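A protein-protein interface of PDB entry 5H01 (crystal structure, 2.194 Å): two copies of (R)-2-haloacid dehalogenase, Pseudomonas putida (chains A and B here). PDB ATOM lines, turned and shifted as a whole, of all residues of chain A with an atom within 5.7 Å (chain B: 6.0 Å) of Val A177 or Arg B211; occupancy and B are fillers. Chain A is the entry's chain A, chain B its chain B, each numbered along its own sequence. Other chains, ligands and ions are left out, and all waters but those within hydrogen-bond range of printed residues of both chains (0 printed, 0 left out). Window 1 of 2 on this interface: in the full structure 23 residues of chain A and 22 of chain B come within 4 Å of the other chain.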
ATOM      1  N   VAL A 175      20.123  -8.935  28.492  1.00  0.00           N
ATOM      2  CA  VAL A 175      19.998  -7.907  27.464  1.00  0.00           C
ATOM      3  C   VAL A 175      20.912  -6.790  27.865  1.00  0.00           C
ATOM      4  O   VAL A 175      20.746  -6.210  28.925  1.00  0.00           O
ATOM      5  CB  VAL A 175      18.536  -7.379  27.302  1.00  0.00           C
ATOM      6  CG1 VAL A 175      18.477  -6.182  26.355  1.00  0.00           C
ATOM      7  CG2 VAL A 175      17.641  -8.486  26.793  1.00  0.00           C
ATOM      8  N   MET A 176      21.904  -6.512  27.035  1.00  0.00           N
ATOM      9  CA  MET A 176      22.858  -5.461  27.331  1.00  0.00           C
ATOM     10  C   MET A 176      22.797  -4.422  26.213  1.00  0.00           C
ATOM     11  O   MET A 176      22.826  -4.760  25.025  1.00  0.00           O
ATOM     12  CB  MET A 176      24.285  -6.047  27.506  1.00  0.00           C
ATOM     13  CG  MET A 176      24.435  -6.981  28.729  1.00  0.00           C
ATOM     14  SD  MET A 176      26.053  -7.776  28.988  1.00  0.00           S
ATOM     15  CE  MET A 176      26.245  -8.715  27.456  1.00  0.00           C
ATOM     16  N   VAL A 177      22.669  -3.155  26.595  1.00  0.00           N
ATOM     17  CA  VAL A 177      22.756  -2.094  25.601  1.00  0.00           C
ATOM     18  C   VAL A 177      24.227  -1.775  25.358  1.00  0.00           C
ATOM     19  O   VAL A 177      24.834  -0.991  26.091  1.00  0.00           O
ATOM     20  CB  VAL A 177      22.008  -0.819  26.033  1.00  0.00           C
ATOM     21  CG1 VAL A 177      22.057   0.228  24.911  1.00  0.00           C
ATOM     22  CG2 VAL A 177      20.553  -1.159  26.422  1.00  0.00           C
ATOM     23  N   GLU A 178      24.792  -2.382  24.325  1.00  0.00           N
ATOM     24  CA  GLU A 178      26.210  -2.196  24.032  1.00  0.00           C
ATOM     25  C   GLU A 178      26.473  -0.742  23.653  1.00  0.00           C
ATOM     26  O   GLU A 178      25.533   0.034  23.447  1.00  0.00           O
ATOM     27  CB  GLU A 178      26.660  -3.152  22.922  1.00  0.00           C
ATOM     28  CG  GLU A 178      26.365  -4.627  23.238  1.00  0.00           C
ATOM     29  CD  GLU A 178      27.217  -5.186  24.378  1.00  0.00           C
ATOM     30  OE1 GLU A 178      28.392  -4.756  24.532  1.00  0.00           O
ATOM     31  OE2 GLU A 178      26.719  -6.079  25.110  1.00  0.00           O
ATOM     32  N   GLU A 179      27.746  -0.372  23.573  1.00  0.00           N
ATOM     33  CA  GLU A 179      28.114   1.032  23.435  1.00  0.00           C
ATOM     34  C   GLU A 179      27.717   1.585  22.093  1.00  0.00           C
ATOM     35  O   GLU A 179      27.476   2.779  21.958  1.00  0.00           O
ATOM     36  CB  GLU A 179      29.617   1.226  23.660  1.00  0.00           C
ATOM     37  CG  GLU A 179      29.953   1.483  25.111  1.00  0.00           C
ATOM     38  CD  GLU A 179      31.312   2.084  25.292  1.00  0.00           C
ATOM     39  OE1 GLU A 179      32.306   1.465  24.856  1.00  0.00           O
ATOM     40  OE2 GLU A 179      31.377   3.192  25.865  1.00  0.00           O
ATOM     41  N   HIS A 181      25.087   0.366  20.582  1.00  0.00           N
ATOM     42  CA  HIS A 181      23.628   0.357  20.728  1.00  0.00           C
ATOM     43  C   HIS A 181      23.156   1.697  21.258  1.00  0.00           C
ATOM     44  O   HIS A 181      22.119   2.224  20.861  1.00  0.00           O
ATOM     45  CB  HIS A 181      23.157  -0.730  21.712  1.00  0.00           C
ATOM     46  CG  HIS A 181      23.471  -2.129  21.295  1.00  0.00           C
ATOM     47  ND1 HIS A 181      22.956  -3.225  21.952  1.00  0.00           N
ATOM     48  CD2 HIS A 181      24.241  -2.616  20.293  1.00  0.00           C
ATOM     49  CE1 HIS A 181      23.377  -4.326  21.362  1.00  0.00           C
ATOM     50  NE2 HIS A 181      24.166  -3.991  20.359  1.00  0.00           N
ATOM     51  N   ALA A 182      23.932   2.215  22.199  1.00  0.00           N
ATOM     52  CA  ALA A 182      23.559   3.378  22.992  1.00  0.00           C
ATOM     53  C   ALA A 182      23.245   4.618  22.156  1.00  0.00           C
ATOM     54  O   ALA A 182      23.881   4.875  21.132  1.00  0.00           O
ATOM     55  CB  ALA A 182      24.683   3.687  23.999  1.00  0.00           C
ATOM     56  N   GLY A 183      22.256   5.385  22.605  1.00  0.00           N
ATOM     57  CA  GLY A 183      21.898   6.643  21.972  1.00  0.00           C
ATOM     58  C   GLY A 183      22.633   7.833  22.569  1.00  0.00           C
ATOM     59  O   GLY A 183      23.842   7.772  22.785  1.00  0.00           O
ATOM     60  N   LEU A 186      22.593   8.501  26.969  1.00  0.00           N
ATOM     61  CA  LEU A 186      23.103   7.245  27.498  1.00  0.00           C
ATOM     62  C   LEU A 186      24.607   7.158  27.218  1.00  0.00           C
ATOM     63  O   LEU A 186      25.369   6.722  28.072  1.00  0.00           O
ATOM     64  CB  LEU A 186      22.333   6.062  26.884  1.00  0.00           C
ATOM     65  CG  LEU A 186      22.524   4.647  27.438  1.00  0.00           C
ATOM     66  CD1 LEU A 186      22.356   4.624  28.951  1.00  0.00           C
ATOM     67  CD2 LEU A 186      21.554   3.681  26.792  1.00  0.00           C
ATOM     68  N   TYR A 190      27.180   6.761  30.050  1.00  0.00           N
ATOM     69  CA  TYR A 190      28.283   5.814  29.918  1.00  0.00           C
ATOM     70  C   TYR A 190      29.619   6.528  30.083  1.00  0.00           C
ATOM     71  O   TYR A 190      30.555   5.997  30.680  1.00  0.00           O
ATOM     72  CB  TYR A 190      28.244   5.108  28.557  1.00  0.00           C
ATOM     73  CG  TYR A 190      27.297   3.928  28.455  1.00  0.00           C
ATOM     74  CD1 TYR A 190      26.509   3.531  29.535  1.00  0.00           C
ATOM     75  CD2 TYR A 190      27.213   3.192  27.279  1.00  0.00           C
ATOM     76  CE1 TYR A 190      25.643   2.435  29.436  1.00  0.00           C
ATOM     77  CE2 TYR A 190      26.355   2.097  27.165  1.00  0.00           C
ATOM     78  CZ  TYR A 190      25.573   1.724  28.239  1.00  0.00           C
ATOM     79  OH  TYR A 190      24.732   0.639  28.106  1.00  0.00           O
ATOM     80  N   LYS A 207      25.571  -2.147  31.443  1.00  0.00           N
ATOM     81  CA  LYS A 207      24.903  -2.340  30.157  1.00  0.00           C
ATOM     82  C   LYS A 207      23.571  -3.070  30.371  1.00  0.00           C
ATOM     83  O   LYS A 207      22.589  -2.789  29.694  1.00  0.00           O
ATOM     84  CB  LYS A 207      25.804  -3.107  29.169  1.00  0.00           C
ATOM     85  CG  LYS A 207      27.161  -2.428  28.901  1.00  0.00           C
ATOM     86  CD  LYS A 207      27.981  -3.110  27.782  1.00  0.00           C
ATOM     87  CE  LYS A 207      28.619  -4.419  28.226  1.00  0.00           C
ATOM     88  NZ  LYS A 207      29.245  -5.181  27.112  1.00  0.00           N
ATOM     89  N   ALA A 208      23.519  -3.989  31.327  1.00  0.00           N
ATOM     90  CA  ALA A 208      22.271  -4.695  31.557  1.00  0.00           C
ATOM     91  C   ALA A 208      21.270  -3.768  32.250  1.00  0.00           C
ATOM     92  O   ALA A 208      20.068  -3.825  31.972  1.00  0.00           O
ATOM     93  CB  ALA A 208      22.491  -5.945  32.367  1.00  0.00           C
ATOM     94  N   ALA A 210      21.150  -0.795  31.649  1.00  0.00           N
ATOM     95  CA  ALA A 210      20.868   0.206  30.626  1.00  0.00           C
ATOM     96  C   ALA A 210      19.604  -0.098  29.817  1.00  0.00           C
ATOM     97  O   ALA A 210      19.148   0.734  29.038  1.00  0.00           O
ATOM     98  CB  ALA A 210      22.056   0.330  29.677  1.00  0.00           C
ATOM     99  N   ARG A 211      19.099  -1.317  29.956  1.00  0.00           N
ATOM    100  CA  ARG A 211      17.887  -1.744  29.299  1.00  0.00           C
ATOM    101  C   ARG A 211      16.777  -0.903  29.922  1.00  0.00           C
ATOM    102  O   ARG A 211      15.817  -0.564  29.259  1.00  0.00           O
ATOM    103  CB  ARG A 211      17.701  -3.255  29.486  1.00  0.00           C
ATOM    104  CG  ARG A 211      16.293  -3.780  29.728  1.00  0.00           C
ATOM    105  CD  ARG A 211      15.452  -3.631  28.525  1.00  0.00           C
ATOM    106  NE  ARG A 211      14.031  -3.944  28.738  1.00  0.00           N
ATOM    107  CZ  ARG A 211      13.087  -3.083  29.087  1.00  0.00           C
ATOM    108  NH1 ARG A 211      13.376  -1.811  29.308  1.00  0.00           N
ATOM    109  NH2 ARG A 211      11.845  -3.513  29.201  1.00  0.00           N
ATOM    110  N   GLU B 116      23.806  -9.686  15.882  1.00  0.00           N
ATOM    111  CA  GLU B 116      22.954  -8.606  16.334  1.00  0.00           C
ATOM    112  C   GLU B 116      21.917  -8.224  15.293  1.00  0.00           C
ATOM    113  O   GLU B 116      20.745  -8.006  15.616  1.00  0.00           O
ATOM    114  CB  GLU B 116      23.815  -7.396  16.695  1.00  0.00           C
ATOM    115  CG  GLU B 116      24.777  -7.662  17.855  1.00  0.00           C
ATOM    116  CD  GLU B 116      25.379  -6.387  18.414  1.00  0.00           C
ATOM    117  OE1 GLU B 116      25.865  -5.563  17.608  1.00  0.00           O
ATOM    118  OE2 GLU B 116      25.347  -6.196  19.658  1.00  0.00           O
ATOM    119  N   GLN B 119      19.198 -10.620  15.256  1.00  0.00           N
ATOM    120  CA  GLN B 119      18.255 -10.414  16.369  1.00  0.00           C
ATOM    121  C   GLN B 119      17.253  -9.302  16.104  1.00  0.00           C
ATOM    122  O   GLN B 119      16.116  -9.353  16.576  1.00  0.00           O
ATOM    123  CB  GLN B 119      19.017 -10.095  17.654  1.00  0.00           C
ATOM    124  CG  GLN B 119      20.094 -11.086  17.939  1.00  0.00           C
ATOM    125  CD  GLN B 119      21.034 -10.628  19.036  1.00  0.00           C
ATOM    126  OE1 GLN B 119      20.631  -9.957  19.984  1.00  0.00           O
ATOM    127  NE2 GLN B 119      22.297 -10.971  18.896  1.00  0.00           N
ATOM    128  N   VAL B 175      11.454  -7.646  24.348  1.00  0.00           N
ATOM    129  CA  VAL B 175      11.981  -6.621  25.236  1.00  0.00           C
ATOM    130  C   VAL B 175      11.590  -5.270  24.692  1.00  0.00           C
ATOM    131  O   VAL B 175      11.937  -4.929  23.569  1.00  0.00           O
ATOM    132  CB  VAL B 175      13.494  -6.698  25.391  1.00  0.00           C
ATOM    133  CG1 VAL B 175      14.007  -5.407  26.002  1.00  0.00           C
ATOM    134  CG2 VAL B 175      13.858  -7.883  26.272  1.00  0.00           C
ATOM    135  N   MET B 176      10.830  -4.521  25.484  1.00  0.00           N
ATOM    136  CA  MET B 176      10.294  -3.244  25.052  1.00  0.00           C
ATOM    137  C   MET B 176      10.743  -2.162  26.010  1.00  0.00           C
ATOM    138  O   MET B 176      10.591  -2.293  27.219  1.00  0.00           O
ATOM    139  CB  MET B 176       8.748  -3.284  24.968  1.00  0.00           C
ATOM    140  CG  MET B 176       8.153  -4.001  23.730  1.00  0.00           C
ATOM    141  SD  MET B 176       6.321  -4.079  23.683  1.00  0.00           S
ATOM    142  CE  MET B 176       5.999  -5.641  24.511  1.00  0.00           C
ATOM    143  N   VAL B 177      11.304  -1.091  25.466  1.00  0.00           N
ATOM    144  CA  VAL B 177      11.621   0.048  26.300  1.00  0.00           C
ATOM    145  C   VAL B 177      10.389   0.950  26.450  1.00  0.00           C
ATOM    146  O   VAL B 177      10.145   1.852  25.636  1.00  0.00           O
ATOM    147  CB  VAL B 177      12.805   0.836  25.742  1.00  0.00           C
ATOM    148  CG1 VAL B 177      13.102   2.030  26.631  1.00  0.00           C
ATOM    149  CG2 VAL B 177      14.044  -0.081  25.646  1.00  0.00           C
ATOM    150  N   TYR B 206       7.967   0.139  18.028  1.00  0.00           N
ATOM    151  CA  TYR B 206       9.101   1.042  18.224  1.00  0.00           C
ATOM    152  C   TYR B 206       9.773   0.778  19.556  1.00  0.00           C
ATOM    153  O   TYR B 206      10.998   0.773  19.647  1.00  0.00           O
ATOM    154  CB  TYR B 206       8.669   2.503  18.121  1.00  0.00           C
ATOM    155  CG  TYR B 206       7.803   2.745  16.920  1.00  0.00           C
ATOM    156  CD1 TYR B 206       8.261   2.472  15.642  1.00  0.00           C
ATOM    157  CD2 TYR B 206       6.510   3.235  17.068  1.00  0.00           C
ATOM    158  CE1 TYR B 206       7.433   2.679  14.527  1.00  0.00           C
ATOM    159  CE2 TYR B 206       5.694   3.447  15.978  1.00  0.00           C
ATOM    160  CZ  TYR B 206       6.154   3.167  14.715  1.00  0.00           C
ATOM    161  OH  TYR B 206       5.311   3.382  13.643  1.00  0.00           O
ATOM    162  N   LYS B 207       8.973   0.535  20.583  1.00  0.00           N
ATOM    163  CA  LYS B 207       9.527   0.254  21.890  1.00  0.00           C
ATOM    164  C   LYS B 207      10.502  -0.921  21.828  1.00  0.00           C
ATOM    165  O   LYS B 207      11.552  -0.864  22.433  1.00  0.00           O
ATOM    166  CB  LYS B 207       8.409  -0.018  22.907  1.00  0.00           C
ATOM    167  CG  LYS B 207       7.468   1.166  23.102  1.00  0.00           C
ATOM    168  CD  LYS B 207       6.509   0.964  24.277  1.00  0.00           C
ATOM    169  CE  LYS B 207       5.783  -0.373  24.202  1.00  0.00           C
ATOM    170  NZ  LYS B 207       4.573  -0.344  25.056  1.00  0.00           N
ATOM    171  N   ALA B 208      10.179  -1.959  21.063  1.00  0.00           N
ATOM    172  CA  ALA B 208      11.059  -3.118  20.967  1.00  0.00           C
ATOM    173  C   ALA B 208      12.278  -2.827  20.088  1.00  0.00           C
ATOM    174  O   ALA B 208      13.350  -3.365  20.313  1.00  0.00           O
ATOM    175  CB  ALA B 208      10.318  -4.313  20.446  1.00  0.00           C
ATOM    176  N   MET B 209      12.117  -1.982  19.077  1.00  0.00           N
ATOM    177  CA  MET B 209      13.274  -1.510  18.346  1.00  0.00           C
ATOM    178  C   MET B 209      14.183  -0.700  19.285  1.00  0.00           C
ATOM    179  O   MET B 209      15.408  -0.712  19.147  1.00  0.00           O
ATOM    180  CB  MET B 209      12.833  -0.678  17.141  1.00  0.00           C
ATOM    181  CG  MET B 209      12.099  -1.489  16.081  1.00  0.00           C
ATOM    182  SD  MET B 209      11.154  -0.529  14.856  1.00  0.00           S
ATOM    183  CE  MET B 209      12.450   0.189  13.802  1.00  0.00           C
ATOM    184  N   ALA B 210      13.584  -0.026  20.263  1.00  0.00           N
ATOM    185  CA  ALA B 210      14.315   0.916  21.114  1.00  0.00           C
ATOM    186  C   ALA B 210      15.377   0.263  22.016  1.00  0.00           C
ATOM    187  O   ALA B 210      16.184   0.954  22.612  1.00  0.00           O
ATOM    188  CB  ALA B 210      13.334   1.698  21.981  1.00  0.00           C
ATOM    189  N   ARG B 211      15.297  -1.023  22.242  1.00  0.00           N
ATOM    190  CA  ARG B 211      16.285  -1.784  22.921  1.00  0.00           C
ATOM    191  C   ARG B 211      17.642  -1.528  22.263  1.00  0.00           C
ATOM    192  O   ARG B 211      18.640  -1.579  22.880  1.00  0.00           O
ATOM    193  CB  ARG B 211      15.851  -3.221  22.842  1.00  0.00           C
ATOM    194  CG  ARG B 211      16.836  -4.226  23.263  1.00  0.00           C
ATOM    195  CD  ARG B 211      17.921  -4.370  22.256  1.00  0.00           C
ATOM    196  NE  ARG B 211      18.927  -5.353  22.624  1.00  0.00           N
ATOM    197  CZ  ARG B 211      20.086  -5.061  23.167  1.00  0.00           C
ATOM    198  NH1 ARG B 211      20.388  -3.854  23.439  1.00  0.00           N
ATOM    199  NH2 ARG B 211      20.926  -5.983  23.458  1.00  0.00           N
ATOM    200  N   TRP B 212      17.583  -1.176  20.993  1.00  0.00           N
ATOM    201  CA  TRP B 212      18.691  -0.814  20.195  1.00  0.00           C
ATOM    202  C   TRP B 212      18.604   0.661  19.786  1.00  0.00           C
ATOM    203  O   TRP B 212      18.401   0.986  18.661  1.00  0.00           O
ATOM    204  CB  TRP B 212      18.743  -1.699  18.973  1.00  0.00           C
ATOM    205  CG  TRP B 212      19.070  -3.074  19.187  1.00  0.00           C
ATOM    206  CD1 TRP B 212      20.276  -3.569  19.484  1.00  0.00           C
ATOM    207  CD2 TRP B 212      18.199  -4.202  19.080  1.00  0.00           C
ATOM    208  NE1 TRP B 212      20.233  -4.923  19.585  1.00  0.00           N
ATOM    209  CE2 TRP B 212      18.965  -5.343  19.339  1.00  0.00           C
ATOM    210  CE3 TRP B 212      16.850  -4.362  18.804  1.00  0.00           C
ATOM    211  CZ2 TRP B 212      18.424  -6.628  19.354  1.00  0.00           C
ATOM    212  CZ3 TRP B 212      16.330  -5.660  18.798  1.00  0.00           C
ATOM    213  CH2 TRP B 212      17.126  -6.753  19.070  1.00  0.00           C
ATOM    214  N   PRO B 213      18.766   1.550  20.734  1.00  0.00           N
ATOM    215  CA  PRO B 213      18.564   2.987  20.500  1.00  0.00           C
ATOM    216  C   PRO B 213      19.123   3.488  19.180  1.00  0.00           C
ATOM    217  O   PRO B 213      18.324   3.922  18.349  1.00  0.00           O
ATOM    218  CB  PRO B 213      19.294   3.641  21.670  1.00  0.00           C
ATOM    219  CG  PRO B 213      19.171   2.631  22.797  1.00  0.00           C
ATOM    220  CD  PRO B 213      19.256   1.280  22.104  1.00  0.00           C
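Val B175 touches its own counterpart, Val A175. Val A175 touches Arg B211, and with the chains exchanged Arg A211 touches Val B175. Met A176 touches Arg B211, and with the chains exchanged Arg A211 touches Met B176. Val A177 touches Arg B211, and with the chains exchanged Arg A211 touches Val B177. 7 positions are printed for both chains.
N of Val A177 is in hydrogen-bond range of O of Lys A207. The backbone NH (N) of Val B177 is in hydrogen-bond range of the backbone carbonyl oxygen (O) of Lys B207 (3.1 Å). The backbone carbonyl oxygen (O) of Val A177 sits at hydrogen-bond distance from the side-chain hydroxyl (OH) of Tyr A190 (2.6 Å). The backbone carbonyl oxygen (O) of Met A176 lies within hydrogen-bond range of a ring nitrogen (ND1) of His A181, 3.4 Å away. ND1 of His A181 sits at hydrogen-bond distance from N of Glu A178, 3.1 Å away.
Of the 13 printed residues of chain B, 7 touch a printed residue of chain A. Printed residues of chain B that touch a printed residue of chain A: Glu B116, Val B175, Met B176, Val B177, Arg B211, Trp B212 and Pro B213. Hydrophobic or aromatic side chains of chain B that line the printed part of chain A: Val B175, Trp B212 and Pro B213. Of the 14 printed residues of chain A, 6 touch a printed residue of chain B. Hydrophobic or aromatic side chains of chain A that line the printed part of chain B: Val A175 and His A181. Along chain A the printed residues that touch a printed residue of chain B span positions 175 to 211. Among the printed residues, 12 pairs touch across the chains. Among the printed residues, no Asp or Glu carboxylate lies within 4 Å of a Lys or Arg side-chain nitrogen of the other chain.
Val A175 touches Val B175 (CG2 to CG2, 3.9 Å). CZ of Arg B211 touches CG1 of Val A175, at 3.7 Å. NH1 of Arg B211 touches CA of Val A177, 3.7 Å away. His A181 touches Trp B212. CB of Pro B213 touches N of Gly A183 (3.6 Å). CG1 of Val B175 touches NE of Arg A211 (3.1 Å). Val B177 touches Arg A211.
Val A177 touches one residue of chain B. Of chain A, only Val A175, Met A176, Val A177 and His A181 come within 4 Å of Arg B211. Of the printed residues of chain A, Pro B213 touches His A181 (3.3 Å) and Gly A183 (3.6 Å). Printed residues of chain B within 4 Å of His A181: Glu B116 (2.6 Å), Arg B211 (3.0 Å), Trp B212 (3.7 Å) and Pro B213 (3.3 Å). Of the printed residues of chain B, Arg A211 touches Val B175 (3.1 Å), Met B176 (2.6 Å) and Val B177 (3.9 Å). Ala B208 touches none of the printed residues of chain A. Glu A179 touches none of the printed residues of chain B. The nearest residue of chain B that does not touch Val A177 is Pro B213 (4.1 Å).
NE2 of His A181 sits at hydrogen-bond distance from OE2 of Glu B116 (2.6 Å). NH2 of Arg B211 lies within hydrogen-bond range of O of Met A176 (2.7 Å). ND1 of His A181 sits at hydrogen-bond distance from NH1 of Arg B211 (3.0 Å). N of Pro B213 sits close to O of His A181 (3.4 Å). The guanidinium group of Arg A211 sits at hydrogen-bond distance from the backbone carbonyl oxygen of Met B176, at 2.6 Å.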
